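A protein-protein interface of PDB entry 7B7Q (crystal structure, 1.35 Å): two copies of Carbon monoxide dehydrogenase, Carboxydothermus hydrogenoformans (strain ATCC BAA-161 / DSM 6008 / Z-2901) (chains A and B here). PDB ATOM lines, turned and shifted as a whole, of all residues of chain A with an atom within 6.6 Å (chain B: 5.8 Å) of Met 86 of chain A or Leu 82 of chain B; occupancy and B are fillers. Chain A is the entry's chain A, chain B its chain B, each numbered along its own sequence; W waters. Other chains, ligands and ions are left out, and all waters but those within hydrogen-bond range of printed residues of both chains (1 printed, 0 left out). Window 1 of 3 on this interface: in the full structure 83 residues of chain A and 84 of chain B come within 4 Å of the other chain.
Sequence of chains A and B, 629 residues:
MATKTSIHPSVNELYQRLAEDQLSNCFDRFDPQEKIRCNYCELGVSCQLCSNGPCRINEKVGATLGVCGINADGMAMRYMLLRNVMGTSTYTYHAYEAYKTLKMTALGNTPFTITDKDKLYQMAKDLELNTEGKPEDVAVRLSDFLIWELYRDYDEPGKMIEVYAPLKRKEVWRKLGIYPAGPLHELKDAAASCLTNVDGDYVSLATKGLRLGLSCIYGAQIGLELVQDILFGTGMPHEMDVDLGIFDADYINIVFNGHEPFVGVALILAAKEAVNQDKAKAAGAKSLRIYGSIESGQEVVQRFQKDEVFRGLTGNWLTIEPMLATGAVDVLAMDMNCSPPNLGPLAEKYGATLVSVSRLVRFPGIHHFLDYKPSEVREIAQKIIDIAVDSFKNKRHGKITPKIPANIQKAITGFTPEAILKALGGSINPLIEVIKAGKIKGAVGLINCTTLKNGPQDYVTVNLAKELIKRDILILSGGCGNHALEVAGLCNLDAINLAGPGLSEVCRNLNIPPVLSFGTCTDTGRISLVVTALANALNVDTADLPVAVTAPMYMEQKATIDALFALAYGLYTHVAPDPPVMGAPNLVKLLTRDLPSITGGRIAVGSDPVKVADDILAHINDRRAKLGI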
ATOM      1  N   TYR A  79       2.323   6.157 -19.704  1.00  0.00           N
ATOM      2  CA  TYR A  79       1.365   5.626 -20.682  1.00  0.00           C
ATOM      3  C   TYR A  79       1.842   5.916 -22.100  1.00  0.00           C
ATOM      4  O   TYR A  79       1.709   5.071 -22.995  1.00  0.00           O
ATOM      5  CB  TYR A  79      -0.036   6.171 -20.401  1.00  0.00           C
ATOM      6  CG  TYR A  79      -1.247   5.412 -20.959  1.00  0.00           C
ATOM      7  CD1 TYR A  79      -1.112   4.257 -21.717  1.00  0.00           C
ATOM      8  CD2 TYR A  79      -2.532   5.873 -20.692  1.00  0.00           C
ATOM      9  CE1 TYR A  79      -2.253   3.594 -22.196  1.00  0.00           C
ATOM     10  CE2 TYR A  79      -3.651   5.218 -21.159  1.00  0.00           C
ATOM     11  CZ  TYR A  79      -3.511   4.078 -21.925  1.00  0.00           C
ATOM     12  OH  TYR A  79      -4.629   3.413 -22.419  1.00  0.00           O
ATOM     13  N   LEU A  81       5.013   5.957 -22.975  1.00  0.00           N
ATOM     14  CA  LEU A  81       6.042   4.934 -23.234  1.00  0.00           C
ATOM     15  C   LEU A  81       5.425   3.569 -23.557  1.00  0.00           C
ATOM     16  O   LEU A  81       5.836   2.908 -24.524  1.00  0.00           O
ATOM     17  CB  LEU A  81       7.011   4.848 -22.047  1.00  0.00           C
ATOM     18  CG  LEU A  81       8.216   3.917 -22.225  1.00  0.00           C
ATOM     19  CD1 LEU A  81       9.124   4.339 -23.378  1.00  0.00           C
ATOM     20  CD2 LEU A  81       9.030   3.844 -20.934  1.00  0.00           C
ATOM     21  N   LEU A  82       4.411   3.155 -22.790  1.00  0.00           N
ATOM     22  CA  LEU A  82       3.754   1.867 -23.034  1.00  0.00           C
ATOM     23  C   LEU A  82       3.159   1.821 -24.435  1.00  0.00           C
ATOM     24  O   LEU A  82       3.315   0.826 -25.161  1.00  0.00           O
ATOM     25  CB  LEU A  82       2.680   1.629 -21.977  1.00  0.00           C
ATOM     26  CG  LEU A  82       1.840   0.354 -22.140  1.00  0.00           C
ATOM     27  CD1 LEU A  82       2.665  -0.891 -22.071  1.00  0.00           C
ATOM     28  CD2 LEU A  82       0.751   0.310 -21.065  1.00  0.00           C
ATOM     29  N   ARG A  83       2.454   2.883 -24.842  1.00  0.00           N
ATOM     30  CA  ARG A  83       1.887   2.869 -26.194  1.00  0.00           C
ATOM     31  C   ARG A  83       2.977   2.810 -27.261  1.00  0.00           C
ATOM     32  O   ARG A  83       2.805   2.157 -28.297  1.00  0.00           O
ATOM     33  CB  ARG A  83       0.943   4.063 -26.420  1.00  0.00           C
ATOM     34  CG  ARG A  83      -0.335   4.007 -25.552  1.00  0.00           C
ATOM     35  CD  ARG A  83      -1.344   5.092 -25.891  1.00  0.00           C
ATOM     36  NE  ARG A  83      -0.788   6.383 -25.539  1.00  0.00           N
ATOM     37  CZ  ARG A  83      -1.179   7.145 -24.524  1.00  0.00           C
ATOM     38  NH1 ARG A  83      -2.283   6.886 -23.854  1.00  0.00           N
ATOM     39  NH2 ARG A  83      -0.492   8.229 -24.260  1.00  0.00           N
ATOM     40  N   ASN A  84       4.111   3.464 -27.026  1.00  0.00           N
ATOM     41  CA  ASN A  84       5.200   3.422 -27.991  1.00  0.00           C
ATOM     42  C   ASN A  84       5.913   2.070 -28.027  1.00  0.00           C
ATOM     43  O   ASN A  84       6.577   1.772 -29.028  1.00  0.00           O
ATOM     44  CB  ASN A  84       6.150   4.598 -27.758  1.00  0.00           C
ATOM     45  CG  ASN A  84       5.638   5.870 -28.403  1.00  0.00           C
ATOM     46  OD1 ASN A  84       5.915   6.117 -29.565  1.00  0.00           O
ATOM     47  ND2 ASN A  84       4.823   6.647 -27.681  1.00  0.00           N
ATOM     48  N   VAL A  85       5.726   1.215 -27.014  1.00  0.00           N
ATOM     49  CA  VAL A  85       6.111  -0.186 -27.165  1.00  0.00           C
ATOM     50  C   VAL A  85       5.373  -0.821 -28.346  1.00  0.00           C
ATOM     51  O   VAL A  85       5.942  -1.632 -29.076  1.00  0.00           O
ATOM     52  CB  VAL A  85       5.880  -0.944 -25.841  1.00  0.00           C
ATOM     53  CG1 VAL A  85       6.043  -2.454 -26.019  1.00  0.00           C
ATOM     54  CG2 VAL A  85       6.837  -0.461 -24.754  1.00  0.00           C
ATOM     55  N   MET A  86       4.074  -0.528 -28.502  1.00  0.00           N
ATOM     56  CA  MET A  86       3.319  -1.060 -29.641  1.00  0.00           C
ATOM     57  C   MET A  86       3.927  -0.586 -30.955  1.00  0.00           C
ATOM     58  O   MET A  86       4.086  -1.367 -31.906  1.00  0.00           O
ATOM     59  CB  MET A  86       1.823  -0.686 -29.580  1.00  0.00           C
ATOM     60  CG  MET A  86       1.080  -1.091 -28.323  1.00  0.00           C
ATOM     61  SD  MET A  86      -0.693  -0.794 -28.437  1.00  0.00           S
ATOM     62  CE  MET A  86      -0.756   0.953 -28.316  1.00  0.00           C
ATOM     63  N   GLY A  87       4.224   0.720 -31.052  1.00  0.00           N
ATOM     64  CA  GLY A  87       4.816   1.226 -32.284  1.00  0.00           C
ATOM     65  C   GLY A  87       6.124   0.524 -32.620  1.00  0.00           C
ATOM     66  O   GLY A  87       6.356   0.112 -33.760  1.00  0.00           O
ATOM     67  N   THR A  88       7.039   0.459 -31.650  1.00  0.00           N
ATOM     68  CA  THR A  88       8.321  -0.217 -31.853  1.00  0.00           C
ATOM     69  C   THR A  88       8.125  -1.675 -32.239  1.00  0.00           C
ATOM     70  O   THR A  88       8.828  -2.202 -33.122  1.00  0.00           O
ATOM     71  CB  THR A  88       9.176  -0.116 -30.574  1.00  0.00           C
ATOM     72  OG1 THR A  88       9.330   1.267 -30.207  1.00  0.00           O
ATOM     73  CG2 THR A  88      10.550  -0.805 -30.750  1.00  0.00           C
ATOM     74  N   SER A  89       7.138  -2.332 -31.626  1.00  0.00           N
ATOM     75  CA  SER A  89       6.892  -3.742 -31.921  1.00  0.00           C
ATOM     76  C   SER A  89       6.473  -3.956 -33.373  1.00  0.00           C
ATOM     77  O   SER A  89       6.857  -4.961 -33.976  1.00  0.00           O
ATOM     78  CB  SER A  89       5.841  -4.324 -30.965  1.00  0.00           C
ATOM     79  OG  SER A  89       6.324  -4.398 -29.618  1.00  0.00           O
ATOM     80  N   THR A  90       5.673  -3.043 -33.945  1.00  0.00           N
ATOM     81  CA  THR A  90       5.283  -3.210 -35.343  1.00  0.00           C
ATOM     82  C   THR A  90       6.476  -3.063 -36.284  1.00  0.00           C
ATOM     83  O   THR A  90       6.611  -3.850 -37.224  1.00  0.00           O
ATOM     84  CB  THR A  90       4.153  -2.253 -35.747  1.00  0.00           C
ATOM     85  OG1 THR A  90       4.603  -0.897 -35.775  1.00  0.00           O
ATOM     86  CG2 THR A  90       2.975  -2.373 -34.839  1.00  0.00           C
ATOM     87  N   TYR A  91       7.373  -2.104 -36.027  1.00  0.00           N
ATOM     88  CA  TYR A  91       8.558  -1.973 -36.876  1.00  0.00           C
ATOM     89  C   TYR A  91       9.491  -3.179 -36.735  1.00  0.00           C
ATOM     90  O   TYR A  91      10.090  -3.640 -37.725  1.00  0.00           O
ATOM     91  CB  TYR A  91       9.318  -0.687 -36.576  1.00  0.00           C
ATOM     92  CG  TYR A  91       8.642   0.608 -37.032  1.00  0.00           C
ATOM     93  CD1 TYR A  91       8.469   0.893 -38.369  1.00  0.00           C
ATOM     94  CD2 TYR A  91       8.186   1.549 -36.109  1.00  0.00           C
ATOM     95  CE1 TYR A  91       7.887   2.100 -38.776  1.00  0.00           C
ATOM     96  CE2 TYR A  91       7.609   2.741 -36.507  1.00  0.00           C
ATOM     97  CZ  TYR A  91       7.456   3.004 -37.833  1.00  0.00           C
ATOM     98  OH  TYR A  91       6.873   4.190 -38.190  1.00  0.00           O
ATOM     99  N   ALA A 191       8.599  -1.893 -21.685  1.00  0.00           N
ATOM    100  CA  ALA A 191       7.355  -2.455 -21.155  1.00  0.00           C
ATOM    101  C   ALA A 191       7.497  -2.818 -19.684  1.00  0.00           C
ATOM    102  O   ALA A 191       6.594  -2.547 -18.896  1.00  0.00           O
ATOM    103  CB  ALA A 191       6.909  -3.664 -21.981  1.00  0.00           C
ATOM    104  N   LEU A 212      14.183   4.215 -27.117  1.00  0.00           N
ATOM    105  CA  LEU A 212      13.329   3.358 -27.912  1.00  0.00           C
ATOM    106  C   LEU A 212      13.266   3.841 -29.358  1.00  0.00           C
ATOM    107  O   LEU A 212      13.342   3.030 -30.294  1.00  0.00           O
ATOM    108  CB  LEU A 212      11.956   3.342 -27.252  1.00  0.00           C
ATOM    109  CG  LEU A 212      10.999   2.213 -27.561  1.00  0.00           C
ATOM    110  CD1 LEU A 212      11.585   0.846 -27.228  1.00  0.00           C
ATOM    111  CD2 LEU A 212       9.625   2.445 -26.885  1.00  0.00           C
ATOM    112  N   GLN A 557       1.188   5.247 -32.760  1.00  0.00           N
ATOM    113  CA  GLN A 557       2.574   5.269 -32.312  1.00  0.00           C
ATOM    114  C   GLN A 557       3.580   4.814 -33.362  1.00  0.00           C
ATOM    115  O   GLN A 557       4.780   4.859 -33.096  1.00  0.00           O
ATOM    116  CB  GLN A 557       2.711   4.494 -31.004  1.00  0.00           C
ATOM    117  CG  GLN A 557       1.855   5.059 -29.895  1.00  0.00           C
ATOM    118  CD  GLN A 557       0.369   4.686 -30.055  1.00  0.00           C
ATOM    119  OE1 GLN A 557       0.052   3.612 -30.572  1.00  0.00           O
ATOM    120  NE2 GLN A 557      -0.537   5.563 -29.604  1.00  0.00           N
ATOM    121  N   LYS A 558       3.141   4.500 -34.578  1.00  0.00           N
ATOM    122  CA  LYS A 558       4.105   4.477 -35.670  1.00  0.00           C
ATOM    123  C   LYS A 558       4.659   5.871 -35.914  1.00  0.00           C
ATOM    124  O   LYS A 558       5.860   6.038 -36.168  1.00  0.00           O
ATOM    125  CB  LYS A 558       3.493   3.861 -36.933  1.00  0.00           C
ATOM    126  CG  LYS A 558       3.233   2.342 -36.715  1.00  0.00           C
ATOM    127  CD  LYS A 558       3.042   1.544 -37.946  1.00  0.00           C
ATOM    128  CE  LYS A 558       4.348   1.356 -38.659  1.00  0.00           C
ATOM    129  NZ  LYS A 558       4.939   0.009 -38.418  1.00  0.00           N
ATOM    130  N   LEU B  49      -5.882   4.655 -26.927  1.00  0.00           N
ATOM    131  CA  LEU B  49      -4.789   4.149 -27.741  1.00  0.00           C
ATOM    132  C   LEU B  49      -4.473   4.969 -28.991  1.00  0.00           C
ATOM    133  O   LEU B  49      -3.423   4.730 -29.584  1.00  0.00           O
ATOM    134  CB  LEU B  49      -4.973   2.658 -28.085  1.00  0.00           C
ATOM    135  CG  LEU B  49      -5.040   1.681 -26.919  1.00  0.00           C
ATOM    136  CD1 LEU B  49      -5.088   0.246 -27.441  1.00  0.00           C
ATOM    137  CD2 LEU B  49      -3.898   1.874 -25.935  1.00  0.00           C
ATOM    138  N   MET B  77     -10.619  -6.568 -24.151  1.00  0.00           N
ATOM    139  CA  MET B  77      -9.598  -7.619 -24.249  1.00  0.00           C
ATOM    140  C   MET B  77      -8.267  -7.068 -24.746  1.00  0.00           C
ATOM    141  O   MET B  77      -7.196  -7.511 -24.320  1.00  0.00           O
ATOM    142  CB  MET B  77     -10.075  -8.794 -25.097  1.00  0.00           C
ATOM    143  CG  MET B  77      -9.162 -10.030 -25.025  1.00  0.00           C
ATOM    144  SD  MET B  77      -8.958 -10.749 -23.376  1.00  0.00           S
ATOM    145  CE  MET B  77      -7.152 -10.753 -23.206  1.00  0.00           C
ATOM    146  N   ARG B  78      -8.311  -6.074 -25.641  1.00  0.00           N
ATOM    147  CA  ARG B  78      -7.077  -5.511 -26.166  1.00  0.00           C
ATOM    148  C   ARG B  78      -6.263  -4.835 -25.070  1.00  0.00           C
ATOM    149  O   ARG B  78      -5.038  -4.983 -25.025  1.00  0.00           O
ATOM    150  CB  ARG B  78      -7.391  -4.551 -27.315  1.00  0.00           C
ATOM    151  CG  ARG B  78      -6.168  -3.898 -27.928  1.00  0.00           C
ATOM    152  CD  ARG B  78      -6.514  -3.097 -29.186  1.00  0.00           C
ATOM    153  NE  ARG B  78      -7.433  -2.012 -28.859  1.00  0.00           N
ATOM    154  CZ  ARG B  78      -7.878  -1.128 -29.741  1.00  0.00           C
ATOM    155  NH1 ARG B  78      -7.508  -1.207 -31.020  1.00  0.00           N
ATOM    156  NH2 ARG B  78      -8.715  -0.165 -29.362  1.00  0.00           N
ATOM    157  N   TYR B  79      -6.915  -4.032 -24.219  1.00  0.00           N
ATOM    158  CA  TYR B  79      -6.144  -3.365 -23.167  1.00  0.00           C
ATOM    159  C   TYR B  79      -5.627  -4.389 -22.147  1.00  0.00           C
ATOM    160  O   TYR B  79      -4.506  -4.269 -21.640  1.00  0.00           O
ATOM    161  CB  TYR B  79      -6.996  -2.256 -22.523  1.00  0.00           C
ATOM    162  CG  TYR B  79      -6.278  -1.135 -21.739  1.00  0.00           C
ATOM    163  CD1 TYR B  79      -4.903  -1.065 -21.615  1.00  0.00           C
ATOM    164  CD2 TYR B  79      -7.024  -0.114 -21.151  1.00  0.00           C
ATOM    165  CE1 TYR B  79      -4.293  -0.023 -20.908  1.00  0.00           C
ATOM    166  CE2 TYR B  79      -6.439   0.921 -20.462  1.00  0.00           C
ATOM    167  CZ  TYR B  79      -5.068   0.955 -20.315  1.00  0.00           C
ATOM    168  OH  TYR B  79      -4.436   1.959 -19.616  1.00  0.00           O
ATOM    169  N   MET B  80      -6.412  -5.434 -21.863  1.00  0.00           N
ATOM    170  CA  MET B  80      -5.899  -6.530 -21.036  1.00  0.00           C
ATOM    171  C   MET B  80      -4.651  -7.158 -21.655  1.00  0.00           C
ATOM    172  O   MET B  80      -3.646  -7.365 -20.969  1.00  0.00           O
ATOM    173  CB  MET B  80      -6.978  -7.584 -20.795  1.00  0.00           C
ATOM    174  CG  MET B  80      -6.458  -8.799 -20.047  1.00  0.00           C
ATOM    175  SD  MET B  80      -7.785  -9.904 -19.553  1.00  0.00           S
ATOM    176  CE  MET B  80      -6.947 -11.029 -18.449  1.00  0.00           C
ATOM    177  N   LEU B  81      -4.683  -7.443 -22.959  1.00  0.00           N
ATOM    178  CA  LEU B  81      -3.500  -8.019 -23.608  1.00  0.00           C
ATOM    179  C   LEU B  81      -2.287  -7.079 -23.505  1.00  0.00           C
ATOM    180  O   LEU B  81      -1.172  -7.512 -23.180  1.00  0.00           O
ATOM    181  CB  LEU B  81      -3.810  -8.381 -25.067  1.00  0.00           C
ATOM    182  CG  LEU B  81      -2.696  -9.138 -25.818  1.00  0.00           C
ATOM    183  CD1 LEU B  81      -2.399 -10.475 -25.165  1.00  0.00           C
ATOM    184  CD2 LEU B  81      -3.072  -9.326 -27.282  1.00  0.00           C
ATOM    185  N   LEU B  82      -2.483  -5.773 -23.790  1.00  0.00           N
ATOM    186  CA  LEU B  82      -1.374  -4.827 -23.729  1.00  0.00           C
ATOM    187  C   LEU B  82      -0.766  -4.796 -22.328  1.00  0.00           C
ATOM    188  O   LEU B  82       0.456  -4.781 -22.167  1.00  0.00           O
ATOM    189  CB  LEU B  82      -1.857  -3.428 -24.143  1.00  0.00           C
ATOM    190  CG  LEU B  82      -0.820  -2.294 -24.057  1.00  0.00           C
ATOM    191  CD1 LEU B  82       0.355  -2.585 -24.997  1.00  0.00           C
ATOM    192  CD2 LEU B  82      -1.467  -0.954 -24.360  1.00  0.00           C
ATOM    193  N   ARG B  83      -1.605  -4.719 -21.288  1.00  0.00           N
ATOM    194  CA  ARG B  83      -1.032  -4.683 -19.941  1.00  0.00           C
ATOM    195  C   ARG B  83      -0.271  -5.974 -19.636  1.00  0.00           C
ATOM    196  O   ARG B  83       0.751  -5.934 -18.947  1.00  0.00           O
ATOM    197  CB  ARG B  83      -2.105  -4.412 -18.888  1.00  0.00           C
ATOM    198  CG  ARG B  83      -2.713  -3.018 -18.958  1.00  0.00           C
ATOM    199  CD  ARG B  83      -3.691  -2.719 -17.792  1.00  0.00           C
ATOM    200  NE  ARG B  83      -4.871  -3.508 -17.979  1.00  0.00           N
ATOM    201  CZ  ARG B  83      -6.081  -3.042 -18.291  1.00  0.00           C
ATOM    202  NH1 ARG B  83      -6.385  -1.755 -18.227  1.00  0.00           N
ATOM    203  NH2 ARG B  83      -7.034  -3.906 -18.546  1.00  0.00           N
ATOM    204  N   ASN B  84      -0.748  -7.116 -20.153  1.00  0.00           N
ATOM    205  CA  ASN B  84      -0.061  -8.385 -19.937  1.00  0.00           C
ATOM    206  C   ASN B  84       1.260  -8.507 -20.702  1.00  0.00           C
ATOM    207  O   ASN B  84       2.111  -9.327 -20.329  1.00  0.00           O
ATOM    208  CB  ASN B  84      -1.016  -9.547 -20.148  1.00  0.00           C
ATOM    209  CG  ASN B  84      -1.853  -9.804 -18.920  1.00  0.00           C
ATOM    210  OD1 ASN B  84      -1.448 -10.528 -18.025  1.00  0.00           O
ATOM    211  ND2 ASN B  84      -3.012  -9.141 -18.830  1.00  0.00           N
ATOM    212  N   VAL B  85       1.474  -7.685 -21.724  1.00  0.00           N
ATOM    213  CA  VAL B  85       2.820  -7.545 -22.284  1.00  0.00           C
ATOM    214  C   VAL B  85       3.795  -7.057 -21.218  1.00  0.00           C
ATOM    215  O   VAL B  85       4.944  -7.496 -21.167  1.00  0.00           O
ATOM    216  CB  VAL B  85       2.786  -6.607 -23.504  1.00  0.00           C
ATOM    217  CG1 VAL B  85       4.198  -6.224 -23.951  1.00  0.00           C
ATOM    218  CG2 VAL B  85       1.987  -7.241 -24.647  1.00  0.00           C
ATOM    219  N   MET B  86       3.352  -6.143 -20.340  1.00  0.00           N
ATOM    220  CA  MET B  86       4.240  -5.675 -19.267  1.00  0.00           C
ATOM    221  C   MET B  86       4.589  -6.822 -18.322  1.00  0.00           C
ATOM    222  O   MET B  86       5.748  -6.980 -17.927  1.00  0.00           O
ATOM    223  CB  MET B  86       3.623  -4.523 -18.455  1.00  0.00           C
ATOM    224  CG  MET B  86       3.256  -3.243 -19.231  1.00  0.00           C
ATOM    225  SD  MET B  86       2.720  -1.893 -18.173  1.00  0.00           S
ATOM    226  CE  MET B  86       1.135  -2.457 -17.611  1.00  0.00           C
ATOM    227  N   ALA B 191       2.035  -7.067 -28.488  1.00  0.00           N
ATOM    228  CA  ALA B 191       2.028  -5.602 -28.495  1.00  0.00           C
ATOM    229  C   ALA B 191       1.663  -5.059 -29.874  1.00  0.00           C
ATOM    230  O   ALA B 191       0.901  -4.097 -29.971  1.00  0.00           O
ATOM    231  CB  ALA B 191       3.393  -5.073 -28.060  1.00  0.00           C
ATOM    232  N   ALA B 192       2.230  -5.629 -30.953  1.00  0.00           N
ATOM    233  CA  ALA B 192       1.896  -5.181 -32.314  1.00  0.00           C
ATOM    234  C   ALA B 192       0.411  -5.364 -32.605  1.00  0.00           C
ATOM    235  O   ALA B 192      -0.198  -4.536 -33.297  1.00  0.00           O
ATOM    236  CB  ALA B 192       2.758  -5.923 -33.329  1.00  0.00           C
ATOM    237  N   CYS B 194      -2.020  -5.029 -30.620  1.00  0.00           N
ATOM    238  CA  CYS B 194      -2.831  -4.071 -29.881  1.00  0.00           C
ATOM    239  C   CYS B 194      -2.808  -2.667 -30.483  1.00  0.00           C
ATOM    240  O   CYS B 194      -3.584  -1.793 -30.064  1.00  0.00           O
ATOM    241  CB  CYS B 194      -2.331  -4.017 -28.429  1.00  0.00           C
ATOM    242  SG  CYS B 194      -2.650  -5.500 -27.444  1.00  0.00           S
ATOM    243  N   LEU B 195      -1.907  -2.406 -31.442  1.00  0.00           N
ATOM    244  CA  LEU B 195      -1.905  -1.100 -32.088  1.00  0.00           C
ATOM    245  C   LEU B 195      -3.243  -0.876 -32.791  1.00  0.00           C
ATOM    246  O   LEU B 195      -3.884  -1.813 -33.267  1.00  0.00           O
ATOM    247  CB  LEU B 195      -0.734  -1.013 -33.089  1.00  0.00           C
ATOM    248  CG  LEU B 195      -0.419   0.395 -33.627  1.00  0.00           C
ATOM    249  CD1 LEU B 195       0.753   1.000 -32.911  1.00  0.00           C
ATOM    250  CD2 LEU B 195      -0.144   0.350 -35.116  1.00  0.00           C
ATOM    251  N   THR B 196      -3.669   0.378 -32.843  1.00  0.00           N
ATOM    252  CA  THR B 196      -4.944   0.700 -33.476  1.00  0.00           C
ATOM    253  C   THR B 196      -5.032   0.095 -34.879  1.00  0.00           C
ATOM    254  O   THR B 196      -4.083   0.130 -35.653  1.00  0.00           O
ATOM    255  CB  THR B 196      -5.123   2.234 -33.511  1.00  0.00           C
ATOM    256  OG1 THR B 196      -5.043   2.732 -32.164  1.00  0.00           O
ATOM    257  CG2 THR B 196      -6.435   2.637 -34.158  1.00  0.00           C
HETATM  258  O   HOH W   1      -2.374   2.441 -31.209  1.00  0.00           O
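The backbone carbonyl oxygen (O) of Cys 194 of chain B sits close to the side-chain sulfur (SD) of Met 86 of chain A. The side-chain sulfur (SD) of Met 86 of chain A lies within hydrogen-bond range of the backbone NH (N) of Leu 195 of chain B (3.6 Å). The side-chain amide nitrogen (NE2) of Gln 557 of chain A is in hydrogen-bond range of the backbone carbonyl oxygen (O) of Leu 49 of chain B, 3.0 Å away. OH of Tyr 79 of chain B sits at hydrogen-bond distance from OH of Tyr 79 of chain A (3.2 Å).
SG of Cys 194 of chain B lies within hydrogen-bond range of O of Arg 78 of chain B. The side-chain hydroxyl of Thr 90 of chain A lies within hydrogen-bond range of the side-chain amino group of Lys 558 of chain A (2.8 Å). The backbone carbonyl oxygen (O) of Val 85 of chain A lies within hydrogen-bond range of the side-chain hydroxyl (OG) of Ser 89 of chain A. The side-chain sulfur (SG) of Cys 194 of chain B sits at hydrogen-bond distance from the backbone NH (N) of Leu 82 of chain B (3.7 Å). The backbone carbonyl oxygen (O) of Gly 87 of chain A lies within hydrogen-bond range of the side-chain hydroxyl (OG1) of Thr 90 of chain A (2.9 Å).
Tyr 79 of chain A touches Leu 49 of chain B. CD1 of Leu 82 of chain A touches CG of Met 86 of chain B, 3.7 Å away. CD1 of Leu 82 of chain B touches CG of Met 86 of chain A, at 3.7 Å. Met 86 of chain A touches Ala 191 of chain B. Gly 87 of chain A touches Leu 195 of chain B (N to CD1, 3.9 Å). Ala 191 of chain B touches Ser 89 of chain A (CB to OG, 3.4 Å). Ala 192 of chain B touches Ser 89 of chain A. Thr 90 of chain A touches Ala 192 of chain B. CG of Met 86 of chain B touches O of Ala 191 of chain A, 3.4 Å away. Gln 557 of chain A touches Leu 195 of chain B.
Printed residues of chain B within 4 Å of Met 86 of chain A: Leu 82 (3.7 Å), Ala 191 (3.4 Å), Cys 194 (3.5 Å) and Leu 195 (3.6 Å). Of chain A, only Met 86 (3.7 Å) comes within 4 Å of Leu 82 of chain B. Printed residues of chain B within 4 Å of Ser 89 of chain A: Ala 191 (3.4 Å) and Ala 192 (3.8 Å). Printed residues of chain A within 4 Å of Ala 191 of chain B: Met 86 (3.4 Å) and Ser 89 (3.4 Å). Printed residues of chain B within 4 Å of Thr 90 of chain A: Ala 192 (3.9 Å). Asn 84 of chain B touches none of the printed residues of chain A. Thr 88 of chain A touches none of the printed residues of chain B. The nearest residue of chain A that does not touch Leu 82 of chain B is Leu 82 of chain A (4.1 Å).
Of the 16 printed residues of chain A, 8 touch a printed residue of chain B. Hydrophobic or aromatic side chains of chain A that line the printed part of chain B: Tyr 79, Leu 82 and Met 86. Of the 16 printed residues of chain B, 8 touch a printed residue of chain A. Printed residues of chain B that touch a printed residue of chain A: Leu 49, Tyr 79, Leu 82, Met 86, Ala 191, Ala 192, Cys 194 and Leu 195. Hydrophobic or aromatic side chains of chain B within 4 Å of the printed part of chain A: Leu 49, Tyr 79, Leu 82, Met 86, Ala 191, Ala 192 and Leu 195. Among the printed residues, no Asp or Glu carboxylate lies within 4 Å of a Lys or Arg side-chain nitrogen of the other chain.
Tyr 79 of chain A touches its own counterpart, Tyr 79 of chain B. Leu 82 of chain A touches Met 86 of chain B, and with the chains exchanged Met 86 of chain A touches Leu 82 of chain B. Met 86 of chain A touches Ala 191 of chain B, and with the chains exchanged Ala 191 of chain A touches Met 86 of chain B.
Water W1 lies within hydrogen-bond range of the side-chain amide oxygen (OE1) of Gln 557 of chain A (2.8 Å), the side-chain hydroxyl (OG1) of Thr 196 of chain B (2.8 Å) and the backbone carbonyl oxygen (O) of Leu 49 of chain B (3.0 Å).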
